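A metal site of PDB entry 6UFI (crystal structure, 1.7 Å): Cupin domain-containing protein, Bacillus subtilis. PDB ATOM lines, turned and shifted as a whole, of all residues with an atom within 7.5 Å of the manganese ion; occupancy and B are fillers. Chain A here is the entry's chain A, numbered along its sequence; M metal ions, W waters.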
ATOM      1  N   VAL A 262     -31.394 -26.005   3.281  1.00  0.00           N
ATOM      2  CA  VAL A 262     -29.943 -26.190   3.348  1.00  0.00           C
ATOM      3  C   VAL A 262     -29.585 -26.848   4.664  1.00  0.00           C
ATOM      4  O   VAL A 262     -30.023 -26.415   5.733  1.00  0.00           O
ATOM      5  CB  VAL A 262     -29.216 -24.834   3.203  1.00  0.00           C
ATOM      6  CG1 VAL A 262     -27.699 -25.041   3.200  1.00  0.00           C
ATOM      7  CG2 VAL A 262     -29.705 -24.110   1.952  1.00  0.00           C
ATOM      8  N   ARG A 270     -22.168 -22.735   4.044  1.00  0.00           N
ATOM      9  CA  ARG A 270     -22.749 -22.367   2.753  1.00  0.00           C
ATOM     10  C   ARG A 270     -21.802 -21.353   2.107  1.00  0.00           C
ATOM     11  O   ARG A 270     -21.499 -20.315   2.711  1.00  0.00           O
ATOM     12  CB  ARG A 270     -24.149 -21.772   2.960  1.00  0.00           C
ATOM     13  CG  ARG A 270     -24.845 -21.243   1.698  1.00  0.00           C
ATOM     14  CD  ARG A 270     -25.542 -22.357   0.916  1.00  0.00           C
ATOM     15  NE  ARG A 270     -26.303 -21.815  -0.218  1.00  0.00           N
ATOM     16  CZ  ARG A 270     -25.781 -21.562  -1.422  1.00  0.00           C
ATOM     17  NH1 ARG A 270     -24.496 -21.807  -1.653  1.00  0.00           N
ATOM     18  NH2 ARG A 270     -26.546 -21.057  -2.388  1.00  0.00           N
ATOM     19  N   GLU A 271     -21.275 -21.671   0.930  1.00  0.00           N
ATOM     20  CA  GLU A 271     -20.149 -20.957   0.339  1.00  0.00           C
ATOM     21  C   GLU A 271     -20.504 -19.504   0.004  1.00  0.00           C
ATOM     22  O   GLU A 271     -21.677 -19.111  -0.038  1.00  0.00           O
ATOM     23  CB  GLU A 271     -19.669 -21.649  -0.936  1.00  0.00           C
ATOM     24  CG  GLU A 271     -20.664 -21.535  -2.083  1.00  0.00           C
ATOM     25  CD  GLU A 271     -20.104 -21.986  -3.429  1.00  0.00           C
ATOM     26  OE1 GLU A 271     -20.928 -22.227  -4.345  1.00  0.00           O
ATOM     27  OE2 GLU A 271     -18.870 -22.087  -3.580  1.00  0.00           O
ATOM     28  N   HIS A 273     -21.521 -16.582  -2.057  1.00  0.00           N
ATOM     29  CA  HIS A 273     -22.370 -16.556  -3.244  1.00  0.00           C
ATOM     30  C   HIS A 273     -23.255 -15.313  -3.187  1.00  0.00           C
ATOM     31  O   HIS A 273     -23.299 -14.616  -2.165  1.00  0.00           O
ATOM     32  CB  HIS A 273     -23.248 -17.812  -3.353  1.00  0.00           C
ATOM     33  CG  HIS A 273     -24.328 -17.910  -2.317  1.00  0.00           C
ATOM     34  ND1 HIS A 273     -24.072 -18.261  -1.005  1.00  0.00           N
ATOM     35  CD2 HIS A 273     -25.663 -17.705  -2.394  1.00  0.00           C
ATOM     36  CE1 HIS A 273     -25.211 -18.271  -0.319  1.00  0.00           C
ATOM     37  NE2 HIS A 273     -26.187 -17.933  -1.142  1.00  0.00           N
ATOM     38  N   TRP A 274     -23.964 -15.055  -4.281  1.00  0.00           N
ATOM     39  CA  TRP A 274     -25.052 -14.089  -4.261  1.00  0.00           C
ATOM     40  C   TRP A 274     -26.166 -14.597  -5.161  1.00  0.00           C
ATOM     41  O   TRP A 274     -26.024 -15.591  -5.879  1.00  0.00           O
ATOM     42  CB  TRP A 274     -24.600 -12.680  -4.677  1.00  0.00           C
ATOM     43  CG  TRP A 274     -24.290 -12.499  -6.147  1.00  0.00           C
ATOM     44  CD1 TRP A 274     -25.127 -12.005  -7.113  1.00  0.00           C
ATOM     45  CD2 TRP A 274     -23.040 -12.772  -6.794  1.00  0.00           C
ATOM     46  NE1 TRP A 274     -24.480 -11.977  -8.332  1.00  0.00           N
ATOM     47  CE2 TRP A 274     -23.199 -12.440  -8.164  1.00  0.00           C
ATOM     48  CE3 TRP A 274     -21.817 -13.282  -6.349  1.00  0.00           C
ATOM     49  CZ2 TRP A 274     -22.162 -12.585  -9.096  1.00  0.00           C
ATOM     50  CZ3 TRP A 274     -20.781 -13.436  -7.288  1.00  0.00           C
ATOM     51  CH2 TRP A 274     -20.969 -13.069  -8.636  1.00  0.00           C
ATOM     52  N   HIS A 275     -27.305 -13.913  -5.099  1.00  0.00           N
ATOM     53  CA  HIS A 275     -28.477 -14.242  -5.915  1.00  0.00           C
ATOM     54  C   HIS A 275     -28.734 -13.136  -6.927  1.00  0.00           C
ATOM     55  O   HIS A 275     -28.947 -11.982  -6.553  1.00  0.00           O
ATOM     56  CB  HIS A 275     -29.690 -14.469  -5.016  1.00  0.00           C
ATOM     57  CG  HIS A 275     -29.450 -15.559  -4.021  1.00  0.00           C
ATOM     58  ND1 HIS A 275     -29.391 -16.885  -4.387  1.00  0.00           N
ATOM     59  CD2 HIS A 275     -29.124 -15.511  -2.705  1.00  0.00           C
ATOM     60  CE1 HIS A 275     -29.071 -17.610  -3.333  1.00  0.00           C
ATOM     61  NE2 HIS A 275     -28.899 -16.797  -2.300  1.00  0.00           N
ATOM     62  N   GLU A 280     -33.167 -12.549  -0.551  1.00  0.00           N
ATOM     63  CA  GLU A 280     -33.283 -13.821   0.173  1.00  0.00           C
ATOM     64  C   GLU A 280     -33.885 -13.583   1.557  1.00  0.00           C
ATOM     65  O   GLU A 280     -33.428 -12.718   2.302  1.00  0.00           O
ATOM     66  CB  GLU A 280     -31.915 -14.496   0.328  1.00  0.00           C
ATOM     67  CG  GLU A 280     -31.956 -15.782   1.175  1.00  0.00           C
ATOM     68  CD  GLU A 280     -30.620 -16.499   1.209  1.00  0.00           C
ATOM     69  OE1 GLU A 280     -29.962 -16.538   0.162  1.00  0.00           O
ATOM     70  OE2 GLU A 280     -30.225 -17.017   2.280  1.00  0.00           O
ATOM     71  N   GLN A 282     -34.712 -15.771   5.136  1.00  0.00           N
ATOM     72  CA  GLN A 282     -34.170 -16.967   5.781  1.00  0.00           C
ATOM     73  C   GLN A 282     -34.972 -17.329   7.015  1.00  0.00           C
ATOM     74  O   GLN A 282     -35.406 -16.451   7.756  1.00  0.00           O
ATOM     75  CB  GLN A 282     -32.720 -16.783   6.247  1.00  0.00           C
ATOM     76  CG  GLN A 282     -31.769 -16.291   5.181  1.00  0.00           C
ATOM     77  CD  GLN A 282     -30.383 -16.041   5.741  1.00  0.00           C
ATOM     78  OE1 GLN A 282     -30.222 -15.675   6.902  1.00  0.00           O
ATOM     79  NE2 GLN A 282     -29.373 -16.233   4.896  1.00  0.00           N
ATOM     80  N   MET A 291     -23.428 -15.038   9.506  1.00  0.00           N
ATOM     81  CA  MET A 291     -23.433 -14.635   8.110  1.00  0.00           C
ATOM     82  C   MET A 291     -22.937 -13.199   8.032  1.00  0.00           C
ATOM     83  O   MET A 291     -23.379 -12.359   8.804  1.00  0.00           O
ATOM     84  CB  MET A 291     -24.854 -14.712   7.514  1.00  0.00           C
ATOM     85  CG  MET A 291     -24.994 -13.933   6.203  1.00  0.00           C
ATOM     86  SD  MET A 291     -26.604 -14.187   5.390  1.00  0.00           S
ATOM     87  CE  MET A 291     -27.712 -13.268   6.462  1.00  0.00           C
ATOM     88  N   VAL A 313     -31.251 -11.274   3.204  1.00  0.00           N
ATOM     89  CA  VAL A 313     -30.147 -10.783   2.383  1.00  0.00           C
ATOM     90  C   VAL A 313     -30.741  -9.978   1.242  1.00  0.00           C
ATOM     91  O   VAL A 313     -31.312 -10.563   0.308  1.00  0.00           O
ATOM     92  CB  VAL A 313     -29.269 -11.915   1.821  1.00  0.00           C
ATOM     93  CG1 VAL A 313     -28.050 -11.333   1.075  1.00  0.00           C
ATOM     94  CG2 VAL A 313     -28.790 -12.857   2.927  1.00  0.00           C
ATOM     95  N   MET A 317     -26.725  -8.937  -2.628  1.00  0.00           N
ATOM     96  CA  MET A 317     -25.619  -8.768  -1.683  1.00  0.00           C
ATOM     97  C   MET A 317     -24.877 -10.092  -1.483  1.00  0.00           C
ATOM     98  O   MET A 317     -25.478 -11.156  -1.410  1.00  0.00           O
ATOM     99  CB  MET A 317     -26.127  -8.232  -0.346  1.00  0.00           C
ATOM    100  CG  MET A 317     -26.701  -6.812  -0.493  1.00  0.00           C
ATOM    101  SD  MET A 317     -26.983  -6.022   1.094  1.00  0.00           S
ATOM    102  CE  MET A 317     -27.513  -4.397   0.545  1.00  0.00           C
ATOM    103  N   HIS A 319     -22.820 -13.038   0.342  1.00  0.00           N
ATOM    104  CA  HIS A 319     -22.971 -13.610   1.681  1.00  0.00           C
ATOM    105  C   HIS A 319     -22.478 -15.057   1.709  1.00  0.00           C
ATOM    106  O   HIS A 319     -22.211 -15.678   0.683  1.00  0.00           O
ATOM    107  CB  HIS A 319     -24.428 -13.531   2.146  1.00  0.00           C
ATOM    108  CG  HIS A 319     -25.415 -14.172   1.230  1.00  0.00           C
ATOM    109  ND1 HIS A 319     -25.737 -13.642  -0.013  1.00  0.00           N
ATOM    110  CD2 HIS A 319     -26.181 -15.280   1.375  1.00  0.00           C
ATOM    111  CE1 HIS A 319     -26.648 -14.410  -0.594  1.00  0.00           C
ATOM    112  NE2 HIS A 319     -26.943 -15.405   0.227  1.00  0.00           N
ATOM    113  N   TYR A 320     -22.311 -15.553   2.932  1.00  0.00           N
ATOM    114  CA  TYR A 320     -22.037 -16.956   3.224  1.00  0.00           C
ATOM    115  C   TYR A 320     -22.827 -17.275   4.485  1.00  0.00           C
ATOM    116  O   TYR A 320     -23.254 -16.372   5.195  1.00  0.00           O
ATOM    117  CB  TYR A 320     -20.522 -17.209   3.447  1.00  0.00           C
ATOM    118  CG  TYR A 320     -20.041 -16.494   4.680  1.00  0.00           C
ATOM    119  CD1 TYR A 320     -19.631 -15.159   4.617  1.00  0.00           C
ATOM    120  CD2 TYR A 320     -20.077 -17.118   5.936  1.00  0.00           C
ATOM    121  CE1 TYR A 320     -19.235 -14.476   5.766  1.00  0.00           C
ATOM    122  CE2 TYR A 320     -19.691 -16.433   7.084  1.00  0.00           C
ATOM    123  CZ  TYR A 320     -19.268 -15.109   6.988  1.00  0.00           C
ATOM    124  OH  TYR A 320     -18.882 -14.432   8.128  1.00  0.00           O
ATOM    125  N   VAL A 321     -22.998 -18.558   4.804  1.00  0.00           N
ATOM    126  CA  VAL A 321     -23.632 -18.926   6.071  1.00  0.00           C
ATOM    127  C   VAL A 321     -22.782 -20.022   6.711  1.00  0.00           C
ATOM    128  O   VAL A 321     -22.765 -21.152   6.221  1.00  0.00           O
ATOM    129  CB  VAL A 321     -25.085 -19.399   5.918  1.00  0.00           C
ATOM    130  CG1 VAL A 321     -25.731 -19.577   7.316  1.00  0.00           C
ATOM    131  CG2 VAL A 321     -25.901 -18.406   5.056  1.00  0.00           C
ATOM    132  N   PHE A 331     -31.410 -24.541   7.604  1.00  0.00           N
ATOM    133  CA  PHE A 331     -32.161 -23.312   7.377  1.00  0.00           C
ATOM    134  C   PHE A 331     -32.789 -23.331   5.990  1.00  0.00           C
ATOM    135  O   PHE A 331     -32.421 -24.126   5.120  1.00  0.00           O
ATOM    136  CB  PHE A 331     -31.275 -22.056   7.580  1.00  0.00           C
ATOM    137  CG  PHE A 331     -30.152 -21.903   6.586  1.00  0.00           C
ATOM    138  CD1 PHE A 331     -28.928 -22.548   6.786  1.00  0.00           C
ATOM    139  CD2 PHE A 331     -30.279 -21.066   5.485  1.00  0.00           C
ATOM    140  CE1 PHE A 331     -27.865 -22.388   5.878  1.00  0.00           C
ATOM    141  CE2 PHE A 331     -29.215 -20.892   4.575  1.00  0.00           C
ATOM    142  CZ  PHE A 331     -28.016 -21.569   4.783  1.00  0.00           C
ATOM    143  N   GLU A 333     -33.788 -20.974   2.577  1.00  0.00           N
ATOM    144  CA  GLU A 333     -33.587 -19.788   1.735  1.00  0.00           C
ATOM    145  C   GLU A 333     -34.845 -19.597   0.910  1.00  0.00           C
ATOM    146  O   GLU A 333     -35.226 -20.501   0.163  1.00  0.00           O
ATOM    147  CB  GLU A 333     -32.380 -19.950   0.801  1.00  0.00           C
ATOM    148  CG  GLU A 333     -31.065 -20.429   1.438  1.00  0.00           C
ATOM    149  CD  GLU A 333     -30.038 -20.841   0.388  1.00  0.00           C
ATOM    150  OE1 GLU A 333     -30.450 -21.282  -0.707  1.00  0.00           O
ATOM    151  OE2 GLU A 333     -28.815 -20.722   0.644  1.00  0.00           O
ATOM    152  N   PHE A 335     -37.241 -17.043  -1.728  1.00  0.00           N
ATOM    153  CA  PHE A 335     -37.150 -15.992  -2.734  1.00  0.00           C
ATOM    154  C   PHE A 335     -38.503 -15.737  -3.368  1.00  0.00           C
ATOM    155  O   PHE A 335     -39.197 -16.682  -3.745  1.00  0.00           O
ATOM    156  CB  PHE A 335     -36.151 -16.369  -3.841  1.00  0.00           C
ATOM    157  CG  PHE A 335     -34.829 -16.807  -3.314  1.00  0.00           C
ATOM    158  CD1 PHE A 335     -34.626 -18.113  -2.917  1.00  0.00           C
ATOM    159  CD2 PHE A 335     -33.795 -15.884  -3.170  1.00  0.00           C
ATOM    160  CE1 PHE A 335     -33.401 -18.524  -2.389  1.00  0.00           C
ATOM    161  CE2 PHE A 335     -32.580 -16.286  -2.637  1.00  0.00           C
ATOM    162  CZ  PHE A 335     -32.395 -17.591  -2.256  1.00  0.00           C
ATOM    163  N   TYR A 340     -35.117 -20.455  -8.510  1.00  0.00           N
ATOM    164  CA  TYR A 340     -33.936 -20.292  -7.684  1.00  0.00           C
ATOM    165  C   TYR A 340     -32.740 -20.027  -8.582  1.00  0.00           C
ATOM    166  O   TYR A 340     -32.577 -20.685  -9.623  1.00  0.00           O
ATOM    167  CB  TYR A 340     -33.708 -21.567  -6.873  1.00  0.00           C
ATOM    168  CG  TYR A 340     -32.509 -21.500  -5.965  1.00  0.00           C
ATOM    169  CD1 TYR A 340     -31.232 -21.798  -6.428  1.00  0.00           C
ATOM    170  CD2 TYR A 340     -32.660 -21.121  -4.639  1.00  0.00           C
ATOM    171  CE1 TYR A 340     -30.133 -21.708  -5.590  1.00  0.00           C
ATOM    172  CE2 TYR A 340     -31.562 -21.037  -3.793  1.00  0.00           C
ATOM    173  CZ  TYR A 340     -30.314 -21.332  -4.274  1.00  0.00           C
ATOM    174  OH  TYR A 340     -29.238 -21.253  -3.423  1.00  0.00           O
ATOM    175  N   ALA A 341     -31.904 -19.071  -8.191  1.00  0.00           N
ATOM    176  CA  ALA A 341     -30.667 -18.821  -8.932  1.00  0.00           C
ATOM    177  C   ALA A 341     -29.592 -18.331  -7.978  1.00  0.00           C
ATOM    178  O   ALA A 341     -29.875 -17.499  -7.109  1.00  0.00           O
ATOM    179  CB  ALA A 341     -30.869 -17.773 -10.033  1.00  0.00           C
ATOM    180  N   ASP A 342     -28.353 -18.816  -8.156  1.00  0.00           N
ATOM    181  CA  ASP A 342     -27.233 -18.250  -7.418  1.00  0.00           C
ATOM    182  C   ASP A 342     -26.003 -18.205  -8.319  1.00  0.00           C
ATOM    183  O   ASP A 342     -25.920 -18.900  -9.329  1.00  0.00           O
ATOM    184  CB  ASP A 342     -26.927 -18.985  -6.086  1.00  0.00           C
ATOM    185  CG  ASP A 342     -26.512 -20.446  -6.272  1.00  0.00           C
ATOM    186  OD1 ASP A 342     -26.593 -21.013  -7.384  1.00  0.00           O
ATOM    187  OD2 ASP A 342     -26.134 -21.067  -5.251  1.00  0.00           O
HETATM  188 MN    MN M   1     -28.120 -17.233  -0.360  1.00  0.00          MN
HETATM  189  O   HOH W   1     -27.929 -18.273   1.525  1.00  0.00           O
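The side-chain carboxylate (OE2) of Glu 280 is in hydrogen-bond range of the side-chain amide nitrogen (NE2) of Gln 282 (2.9 Å).
NE2 of His 273 lies close to NH2 of Arg 270, 3.4 Å away.
The backbone carbonyl oxygen (O) of Glu 271 is in hydrogen-bond range of a ring nitrogen (ND1) of His 273, 2.7 Å away.
A ring nitrogen (ND1) of His 275 lies within hydrogen-bond range of the backbone carbonyl oxygen (O) of Ala 341.
The guanidinium group (NE) of Arg 270 lies within salt-bridge range of the side-chain carboxylate (OE2) of Glu 333.
ND1 of His 319 is in hydrogen-bond range of O of Met 317 (2.9 Å).
The backbone carbonyl oxygen of Glu 280 sits at hydrogen-bond distance from the backbone NH of Val 313, at 2.8 Å.
The side-chain hydroxyl (OH) of Tyr 340 is in hydrogen-bond range of the side-chain carboxylate (OE1) of Glu 333, 3.0 Å away.
The manganese ion is bound by OE1 of Glu 280 (2.0 Å), NE2 of His 275 (2.1 Å), water W1 (2.2 Å), NE2 of His 273 (2.2 Å) and NE2 of His 319 (2.3 Å).
The manganese ion has five donor atoms within binding distance.
Glu 333 touches the manganese ion.
Five residues have an atom within 4 Å of the manganese ion: His 273, His 275, Glu 280, His 319 and Glu 333.
Along chain A the residues within 4 Å of the manganese ion span positions 273 to 333.
The nearest printed residue that does not touch the manganese ion is Arg 270 (4.6 Å).
Water W1 lies within hydrogen-bond range of the side-chain carboxylate (OE2) of Glu 280 (2.7 Å) and the side-chain carboxylate (OE2) of Glu 333 (2.7 Å).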
